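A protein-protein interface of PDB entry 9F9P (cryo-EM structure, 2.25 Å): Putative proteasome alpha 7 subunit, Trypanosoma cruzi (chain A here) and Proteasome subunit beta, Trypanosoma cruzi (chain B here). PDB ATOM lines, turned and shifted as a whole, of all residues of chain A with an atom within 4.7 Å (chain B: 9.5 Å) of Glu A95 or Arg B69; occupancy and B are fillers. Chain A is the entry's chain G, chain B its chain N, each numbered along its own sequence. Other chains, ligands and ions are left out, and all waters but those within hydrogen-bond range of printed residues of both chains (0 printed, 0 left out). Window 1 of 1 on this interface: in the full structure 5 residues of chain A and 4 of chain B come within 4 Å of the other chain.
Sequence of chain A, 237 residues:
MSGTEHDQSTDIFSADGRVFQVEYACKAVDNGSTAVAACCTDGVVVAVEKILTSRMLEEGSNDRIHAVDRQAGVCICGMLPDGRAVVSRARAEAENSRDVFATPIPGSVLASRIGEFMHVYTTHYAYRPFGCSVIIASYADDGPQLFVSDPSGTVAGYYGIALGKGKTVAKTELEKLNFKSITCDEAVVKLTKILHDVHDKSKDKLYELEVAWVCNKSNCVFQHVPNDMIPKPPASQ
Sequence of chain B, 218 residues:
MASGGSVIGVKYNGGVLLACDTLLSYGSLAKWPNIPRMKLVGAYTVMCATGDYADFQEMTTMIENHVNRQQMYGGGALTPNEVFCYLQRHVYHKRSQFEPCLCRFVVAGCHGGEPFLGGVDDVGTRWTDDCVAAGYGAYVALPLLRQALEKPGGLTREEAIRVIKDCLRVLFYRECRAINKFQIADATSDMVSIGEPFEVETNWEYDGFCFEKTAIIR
The backbone carbonyl oxygen of Thr B61 sits close to the side-chain amide nitrogen of Asn B65, at 3.3 Å.
Of the 9 printed residues of chain A, 3 touch a printed residue of chain B.
Hydrophobic or aromatic side chains of chain B that line the printed part of chain A: Tyr B73.
Among the printed residues, 5 pairs touch across the chains.
Of chain B, only Arg B69 and Tyr B73 come within 4 Å of Glu A95.
Arg B69 touches just these residues of chain A: Glu A95 and Asp A99.
No residue of chain B comes within 4 Å of Ala A92.
Ala A94 touches none of the printed residues of chain B.
Of the printed residues of chain B, Asp A99 touches Asn B65 and Arg B69.
Printed residues of chain A within 4 Å of Tyr B73: Arg A91 (3.5 Å) and Glu A95 (2.5 Å).
Of the printed residues of chain A, Asn B65 touches Asp A99 (3.2 Å).
Printed residues of chain B within 4 Å of Arg A91: Tyr B73 (3.5 Å).
Glu A93 touches none of the printed residues of chain B.
Gln B70 touches none of the printed residues of chain A.
The nearest residue of chain B that does not touch Glu A95 is Met B72 (6.6 Å).
The nearest printed residue of chain A that does not touch Asn B65 is Arg A98 (6.2 Å).
Tyr B73 touches Arg A91 (CD1 to NE, 3.5 Å).
Glu A95 touches Arg B69 (CG to CZ, 3.4 Å).
The side-chain amide nitrogen of Asn B65 is in hydrogen-bond range of the side-chain carboxylate of Asp A99, at 3.2 Å.
The guanidinium group of Arg B69 lies within salt-bridge range of the side-chain carboxylate of Asp A99 (3.0 Å).
The side-chain hydroxyl of Tyr B73 sits at hydrogen-bond distance from the side-chain carboxylate of Glu A95, 2.5 Å away.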
ATOM      1  N   ARG A  91       2.536   1.331  17.898  1.00  0.00           N
ATOM      2  CA  ARG A  91       2.520   2.784  18.005  1.00  0.00           C
ATOM      3  C   ARG A  91       3.225   3.388  16.795  1.00  0.00           C
ATOM      4  O   ARG A  91       2.721   4.339  16.205  1.00  0.00           O
ATOM      5  CB  ARG A  91       3.160   3.253  19.327  1.00  0.00           C
ATOM      6  CG  ARG A  91       2.131   3.299  20.461  1.00  0.00           C
ATOM      7  CD  ARG A  91       2.730   3.411  21.823  1.00  0.00           C
ATOM      8  NE  ARG A  91       1.646   3.338  22.786  1.00  0.00           N
ATOM      9  CZ  ARG A  91       1.821   3.476  24.102  1.00  0.00           C
ATOM     10  NH1 ARG A  91       3.030   3.653  24.591  1.00  0.00           N
ATOM     11  NH2 ARG A  91       0.784   3.508  24.907  1.00  0.00           N
ATOM     12  N   ALA A  92       4.375   2.845  16.422  1.00  0.00           N
ATOM     13  CA  ALA A  92       5.121   3.319  15.263  1.00  0.00           C
ATOM     14  C   ALA A  92       4.375   3.137  13.922  1.00  0.00           C
ATOM     15  O   ALA A  92       4.443   4.029  13.085  1.00  0.00           O
ATOM     16  CB  ALA A  92       6.432   2.600  15.227  1.00  0.00           C
ATOM     17  N   GLU A  93       3.712   2.001  13.677  1.00  0.00           N
ATOM     18  CA  GLU A  93       2.857   1.789  12.512  1.00  0.00           C
ATOM     19  C   GLU A  93       1.647   2.717  12.439  1.00  0.00           C
ATOM     20  O   GLU A  93       1.219   3.085  11.346  1.00  0.00           O
ATOM     21  CB  GLU A  93       2.215   0.386  12.483  1.00  0.00           C
ATOM     22  CG  GLU A  93       3.227  -0.753  12.269  1.00  0.00           C
ATOM     23  CD  GLU A  93       3.996  -0.779  10.937  1.00  0.00           C
ATOM     24  OE1 GLU A  93       3.546  -0.083   9.962  1.00  0.00           O
ATOM     25  OE2 GLU A  93       5.071  -1.471  10.866  1.00  0.00           O
ATOM     26  N   ALA A  94       1.009   3.003  13.560  1.00  0.00           N
ATOM     27  CA  ALA A  94      -0.100   3.937  13.564  1.00  0.00           C
ATOM     28  C   ALA A  94       0.376   5.352  13.227  1.00  0.00           C
ATOM     29  O   ALA A  94      -0.338   6.036  12.488  1.00  0.00           O
ATOM     30  CB  ALA A  94      -0.803   3.927  14.896  1.00  0.00           C
ATOM     31  N   GLU A  95       1.510   5.790  13.773  1.00  0.00           N
ATOM     32  CA  GLU A  95       2.092   7.079  13.433  1.00  0.00           C
ATOM     33  C   GLU A  95       2.504   7.192  11.962  1.00  0.00           C
ATOM     34  O   GLU A  95       2.270   8.208  11.316  1.00  0.00           O
ATOM     35  CB  GLU A  95       3.364   7.333  14.248  1.00  0.00           C
ATOM     36  CG  GLU A  95       3.082   7.644  15.739  1.00  0.00           C
ATOM     37  CD  GLU A  95       4.286   7.430  16.664  1.00  0.00           C
ATOM     38  OE1 GLU A  95       4.116   7.508  17.920  1.00  0.00           O
ATOM     39  OE2 GLU A  95       5.413   7.135  16.132  1.00  0.00           O
ATOM     40  N   ASN A  96       3.163   6.170  11.434  1.00  0.00           N
ATOM     41  CA  ASN A  96       3.486   6.111  10.027  1.00  0.00           C
ATOM     42  C   ASN A  96       2.238   6.280   9.154  1.00  0.00           C
ATOM     43  O   ASN A  96       2.258   6.919   8.115  1.00  0.00           O
ATOM     44  CB  ASN A  96       4.097   4.754   9.689  1.00  0.00           C
ATOM     45  CG  ASN A  96       4.460   4.599   8.231  1.00  0.00           C
ATOM     46  OD1 ASN A  96       3.745   3.989   7.431  1.00  0.00           O
ATOM     47  ND2 ASN A  96       5.583   5.201   7.893  1.00  0.00           N
ATOM     48  N   SER A  97       1.128   5.700   9.537  1.00  0.00           N
ATOM     49  CA  SER A  97      -0.037   5.827   8.690  1.00  0.00           C
ATOM     50  C   SER A  97      -0.551   7.259   8.684  1.00  0.00           C
ATOM     51  O   SER A  97      -0.992   7.743   7.648  1.00  0.00           O
ATOM     52  CB  SER A  97      -1.112   4.862   9.082  1.00  0.00           C
ATOM     53  OG  SER A  97      -2.359   5.285   8.588  1.00  0.00           O
ATOM     54  N   ARG A  98      -0.522   7.943   9.820  1.00  0.00           N
ATOM     55  CA  ARG A  98      -0.960   9.334   9.861  1.00  0.00           C
ATOM     56  C   ARG A  98       0.007  10.255   9.128  1.00  0.00           C
ATOM     57  O   ARG A  98      -0.447  11.123   8.406  1.00  0.00           O
ATOM     58  CB  ARG A  98      -1.129   9.797  11.309  1.00  0.00           C
ATOM     59  CG  ARG A  98      -2.478   9.359  11.863  1.00  0.00           C
ATOM     60  CD  ARG A  98      -2.678   9.708  13.293  1.00  0.00           C
ATOM     61  NE  ARG A  98      -3.920   9.060  13.729  1.00  0.00           N
ATOM     62  CZ  ARG A  98      -5.099   9.655  13.807  1.00  0.00           C
ATOM     63  NH1 ARG A  98      -5.288  10.826  13.242  1.00  0.00           N
ATOM     64  NH2 ARG A  98      -6.102   9.049  14.404  1.00  0.00           N
ATOM     65  N   ASP A  99       1.307  10.056   9.291  1.00  0.00           N
ATOM     66  CA  ASP A  99       2.287  10.976   8.759  1.00  0.00           C
ATOM     67  C   ASP A  99       2.463  10.842   7.243  1.00  0.00           C
ATOM     68  O   ASP A  99       2.566  11.842   6.552  1.00  0.00           O
ATOM     69  CB  ASP A  99       3.619  10.790   9.484  1.00  0.00           C
ATOM     70  CG  ASP A  99       3.558  11.191  10.968  1.00  0.00           C
ATOM     71  OD1 ASP A  99       2.620  11.952  11.351  1.00  0.00           O
ATOM     72  OD2 ASP A  99       4.395  10.675  11.771  1.00  0.00           O
ATOM     73  N   GLY B  42      -1.806  21.410  21.287  1.00  0.00           N
ATOM     74  CA  GLY B  42      -2.153  20.885  22.589  1.00  0.00           C
ATOM     75  C   GLY B  42      -3.292  21.675  23.225  1.00  0.00           C
ATOM     76  O   GLY B  42      -4.177  22.202  22.544  1.00  0.00           O
ATOM     77  N   THR B  61       3.254  20.893  12.264  1.00  0.00           N
ATOM     78  CA  THR B  61       2.784  19.520  12.192  1.00  0.00           C
ATOM     79  C   THR B  61       3.619  18.604  13.109  1.00  0.00           C
ATOM     80  O   THR B  61       3.056  17.824  13.878  1.00  0.00           O
ATOM     81  CB  THR B  61       2.840  19.054  10.726  1.00  0.00           C
ATOM     82  OG1 THR B  61       1.805  19.719  10.009  1.00  0.00           O
ATOM     83  CG2 THR B  61       2.693  17.563  10.574  1.00  0.00           C
ATOM     84  N   MET B  62       4.935  18.752  13.036  1.00  0.00           N
ATOM     85  CA  MET B  62       5.879  18.024  13.847  1.00  0.00           C
ATOM     86  C   MET B  62       5.681  18.302  15.351  1.00  0.00           C
ATOM     87  O   MET B  62       5.691  17.395  16.167  1.00  0.00           O
ATOM     88  CB  MET B  62       7.294  18.406  13.388  1.00  0.00           C
ATOM     89  CG  MET B  62       8.410  17.693  14.092  1.00  0.00           C
ATOM     90  SD  MET B  62       8.761  18.320  15.782  1.00  0.00           S
ATOM     91  CE  MET B  62       9.884  19.697  15.489  1.00  0.00           C
ATOM     92  N   ILE B  63       5.508  19.548  15.762  1.00  0.00           N
ATOM     93  CA  ILE B  63       5.289  19.842  17.164  1.00  0.00           C
ATOM     94  C   ILE B  63       3.943  19.350  17.629  1.00  0.00           C
ATOM     95  O   ILE B  63       3.867  18.871  18.724  1.00  0.00           O
ATOM     96  CB  ILE B  63       5.499  21.351  17.461  1.00  0.00           C
ATOM     97  CG1 ILE B  63       6.978  21.702  17.303  1.00  0.00           C
ATOM     98  CG2 ILE B  63       5.081  21.756  18.863  1.00  0.00           C
ATOM     99  CD1 ILE B  63       7.245  23.215  17.340  1.00  0.00           C
ATOM    100  N   GLU B  64       2.874  19.515  16.865  1.00  0.00           N
ATOM    101  CA  GLU B  64       1.555  19.003  17.247  1.00  0.00           C
ATOM    102  C   GLU B  64       1.503  17.476  17.426  1.00  0.00           C
ATOM    103  O   GLU B  64       0.841  16.975  18.322  1.00  0.00           O
ATOM    104  CB  GLU B  64       0.496  19.247  16.178  1.00  0.00           C
ATOM    105  CG  GLU B  64      -0.110  20.627  16.139  1.00  0.00           C
ATOM    106  CD  GLU B  64      -0.944  20.910  14.867  1.00  0.00           C
ATOM    107  OE1 GLU B  64      -1.568  22.028  14.753  1.00  0.00           O
ATOM    108  OE2 GLU B  64      -0.983  20.016  13.949  1.00  0.00           O
ATOM    109  N   ASN B  65       2.106  16.728  16.523  1.00  0.00           N
ATOM    110  CA  ASN B  65       2.204  15.286  16.687  1.00  0.00           C
ATOM    111  C   ASN B  65       2.932  14.922  17.975  1.00  0.00           C
ATOM    112  O   ASN B  65       2.395  14.085  18.700  1.00  0.00           O
ATOM    113  CB  ASN B  65       2.866  14.607  15.484  1.00  0.00           C
ATOM    114  CG  ASN B  65       1.995  14.701  14.245  1.00  0.00           C
ATOM    115  OD1 ASN B  65       0.788  14.880  14.313  1.00  0.00           O
ATOM    116  ND2 ASN B  65       2.624  14.598  13.102  1.00  0.00           N
ATOM    117  N   HIS B  66       4.089  15.540  18.280  1.00  0.00           N
ATOM    118  CA  HIS B  66       4.795  15.270  19.531  1.00  0.00           C
ATOM    119  C   HIS B  66       3.908  15.566  20.750  1.00  0.00           C
ATOM    120  O   HIS B  66       3.717  14.742  21.627  1.00  0.00           O
ATOM    121  CB  HIS B  66       6.169  15.950  19.565  1.00  0.00           C
ATOM    122  CG  HIS B  66       6.936  15.927  20.877  1.00  0.00           C
ATOM    123  ND1 HIS B  66       7.662  14.840  21.300  1.00  0.00           N
ATOM    124  CD2 HIS B  66       7.129  16.872  21.849  1.00  0.00           C
ATOM    125  CE1 HIS B  66       8.226  15.110  22.477  1.00  0.00           C
ATOM    126  NE2 HIS B  66       7.985  16.365  22.866  1.00  0.00           N
ATOM    127  N   VAL B  67       3.203  16.661  20.755  1.00  0.00           N
ATOM    128  CA  VAL B  67       2.389  16.974  21.899  1.00  0.00           C
ATOM    129  C   VAL B  67       1.212  16.001  22.089  1.00  0.00           C
ATOM    130  O   VAL B  67       0.931  15.612  23.216  1.00  0.00           O
ATOM    131  CB  VAL B  67       1.962  18.452  21.808  1.00  0.00           C
ATOM    132  CG1 VAL B  67       0.894  18.803  22.826  1.00  0.00           C
ATOM    133  CG2 VAL B  67       3.164  19.394  21.989  1.00  0.00           C
ATOM    134  N   ASN B  68       0.449  15.672  21.042  1.00  0.00           N
ATOM    135  CA  ASN B  68      -0.650  14.711  21.141  1.00  0.00           C
ATOM    136  C   ASN B  68      -0.190  13.306  21.557  1.00  0.00           C
ATOM    137  O   ASN B  68      -0.765  12.723  22.459  1.00  0.00           O
ATOM    138  CB  ASN B  68      -1.388  14.567  19.812  1.00  0.00           C
ATOM    139  CG  ASN B  68      -2.074  15.846  19.360  1.00  0.00           C
ATOM    140  OD1 ASN B  68      -2.437  16.699  20.168  1.00  0.00           O
ATOM    141  ND2 ASN B  68      -2.266  15.994  18.058  1.00  0.00           N
ATOM    142  N   ARG B  69       0.919  12.821  20.998  1.00  0.00           N
ATOM    143  CA  ARG B  69       1.455  11.516  21.328  1.00  0.00           C
ATOM    144  C   ARG B  69       1.934  11.422  22.769  1.00  0.00           C
ATOM    145  O   ARG B  69       1.587  10.473  23.453  1.00  0.00           O
ATOM    146  CB  ARG B  69       2.553  11.144  20.328  1.00  0.00           C
ATOM    147  CG  ARG B  69       2.000  10.821  18.940  1.00  0.00           C
ATOM    148  CD  ARG B  69       3.024  10.859  17.810  1.00  0.00           C
ATOM    149  NE  ARG B  69       2.308  10.954  16.522  1.00  0.00           N
ATOM    150  CZ  ARG B  69       2.896  11.042  15.321  1.00  0.00           C
ATOM    151  NH1 ARG B  69       4.210  10.970  15.194  1.00  0.00           N
ATOM    152  NH2 ARG B  69       2.144  11.123  14.232  1.00  0.00           N
ATOM    153  N   GLN B  70       2.747  12.364  23.240  1.00  0.00           N
ATOM    154  CA  GLN B  70       3.214  12.341  24.613  1.00  0.00           C
ATOM    155  C   GLN B  70       2.037  12.258  25.572  1.00  0.00           C
ATOM    156  O   GLN B  70       2.068  11.498  26.509  1.00  0.00           O
ATOM    157  CB  GLN B  70       4.150  13.512  24.900  1.00  0.00           C
ATOM    158  CG  GLN B  70       4.635  13.534  26.341  1.00  0.00           C
ATOM    159  CD  GLN B  70       6.031  14.096  26.538  1.00  0.00           C
ATOM    160  OE1 GLN B  70       6.973  13.738  25.809  1.00  0.00           O
ATOM    161  NE2 GLN B  70       6.186  14.881  27.607  1.00  0.00           N
ATOM    162  N   GLN B  71       0.944  12.935  25.294  1.00  0.00           N
ATOM    163  CA  GLN B  71      -0.220  12.829  26.153  1.00  0.00           C
ATOM    164  C   GLN B  71      -0.946  11.487  26.071  1.00  0.00           C
ATOM    165  O   GLN B  71      -1.399  10.964  27.072  1.00  0.00           O
ATOM    166  CB  GLN B  71      -1.240  13.903  25.820  1.00  0.00           C
ATOM    167  CG  GLN B  71      -1.968  14.340  27.067  1.00  0.00           C
ATOM    168  CD  GLN B  71      -3.443  14.320  26.810  1.00  0.00           C
ATOM    169  OE1 GLN B  71      -3.947  15.006  25.921  1.00  0.00           O
ATOM    170  NE2 GLN B  71      -4.129  13.496  27.582  1.00  0.00           N
ATOM    171  N   MET B  72      -1.117  10.946  24.874  1.00  0.00           N
ATOM    172  CA  MET B  72      -1.794   9.677  24.635  1.00  0.00           C
ATOM    173  C   MET B  72      -1.028   8.488  25.234  1.00  0.00           C
ATOM    174  O   MET B  72      -1.640   7.475  25.526  1.00  0.00           O
ATOM    175  CB  MET B  72      -1.878   9.484  23.123  1.00  0.00           C
ATOM    176  CG  MET B  72      -3.070   8.748  22.600  1.00  0.00           C
ATOM    177  SD  MET B  72      -3.496   9.264  20.891  1.00  0.00           S
ATOM    178  CE  MET B  72      -1.961   8.996  19.983  1.00  0.00           C
ATOM    179  N   TYR B  73       0.304   8.577  25.325  1.00  0.00           N
ATOM    180  CA  TYR B  73       1.166   7.490  25.772  1.00  0.00           C
ATOM    181  C   TYR B  73       1.574   7.666  27.243  1.00  0.00           C
ATOM    182  O   TYR B  73       2.541   7.048  27.664  1.00  0.00           O
ATOM    183  CB  TYR B  73       2.468   7.448  24.949  1.00  0.00           C
ATOM    184  CG  TYR B  73       2.325   7.248  23.446  1.00  0.00           C
ATOM    185  CD1 TYR B  73       1.161   6.773  22.857  1.00  0.00           C
ATOM    186  CD2 TYR B  73       3.394   7.517  22.607  1.00  0.00           C
ATOM    187  CE1 TYR B  73       1.021   6.711  21.480  1.00  0.00           C
ATOM    188  CE2 TYR B  73       3.310   7.395  21.230  1.00  0.00           C
ATOM    189  CZ  TYR B  73       2.109   7.023  20.653  1.00  0.00           C
ATOM    190  OH  TYR B  73       2.075   6.913  19.268  1.00  0.00           O
ATOM    191  N   GLY B  74       0.948   8.595  27.985  1.00  0.00           N
ATOM    192  CA  GLY B  74       1.084   8.682  29.436  1.00  0.00           C
ATOM    193  C   GLY B  74       2.125   9.661  30.024  1.00  0.00           C
ATOM    194  O   GLY B  74       2.323   9.642  31.243  1.00  0.00           O
ATOM    195  N   GLY B  75       2.692  10.589  29.233  1.00  0.00           N
ATOM    196  CA  GLY B  75       3.638  11.590  29.733  1.00  0.00           C
ATOM    197  C   GLY B  75       3.092  13.021  29.914  1.00  0.00           C
ATOM    198  O   GLY B  75       3.875  13.975  29.850  1.00  0.00           O
ATOM    199  N   GLY B  76       1.771  13.193  30.136  1.00  0.00           N
ATOM    200  CA  GLY B  76       1.204  14.473  30.547  1.00  0.00           C
ATOM    201  C   GLY B  76       1.056  15.478  29.397  1.00  0.00           C
ATOM    202  O   GLY B  76       1.468  15.203  28.272  1.00  0.00           O
ATOM    203  N   ALA B  77       0.468  16.655  29.684  1.00  0.00           N
ATOM    204  CA  ALA B  77       0.200  17.675  28.666  1.00  0.00           C
ATOM    205  C   ALA B  77       1.248  18.786  28.719  1.00  0.00           C
ATOM    206  O   ALA B  77       1.378  19.446  29.751  1.00  0.00           O
ATOM    207  CB  ALA B  77      -1.185  18.247  28.896  1.00  0.00           C
ATOM    208  N   LEU B  78       1.995  19.011  27.638  1.00  0.00           N
ATOM    209  CA  LEU B  78       3.027  20.042  27.668  1.00  0.00           C
ATOM    210  C   LEU B  78       2.443  21.452  27.822  1.00  0.00           C
ATOM    211  O   LEU B  78       1.453  21.796  27.173  1.00  0.00           O
ATOM    212  CB  LEU B  78       3.851  19.941  26.386  1.00  0.00           C
ATOM    213  CG  LEU B  78       4.697  18.664  26.287  1.00  0.00           C
ATOM    214  CD1 LEU B  78       5.574  18.687  25.043  1.00  0.00           C
ATOM    215  CD2 LEU B  78       5.554  18.494  27.518  1.00  0.00           C
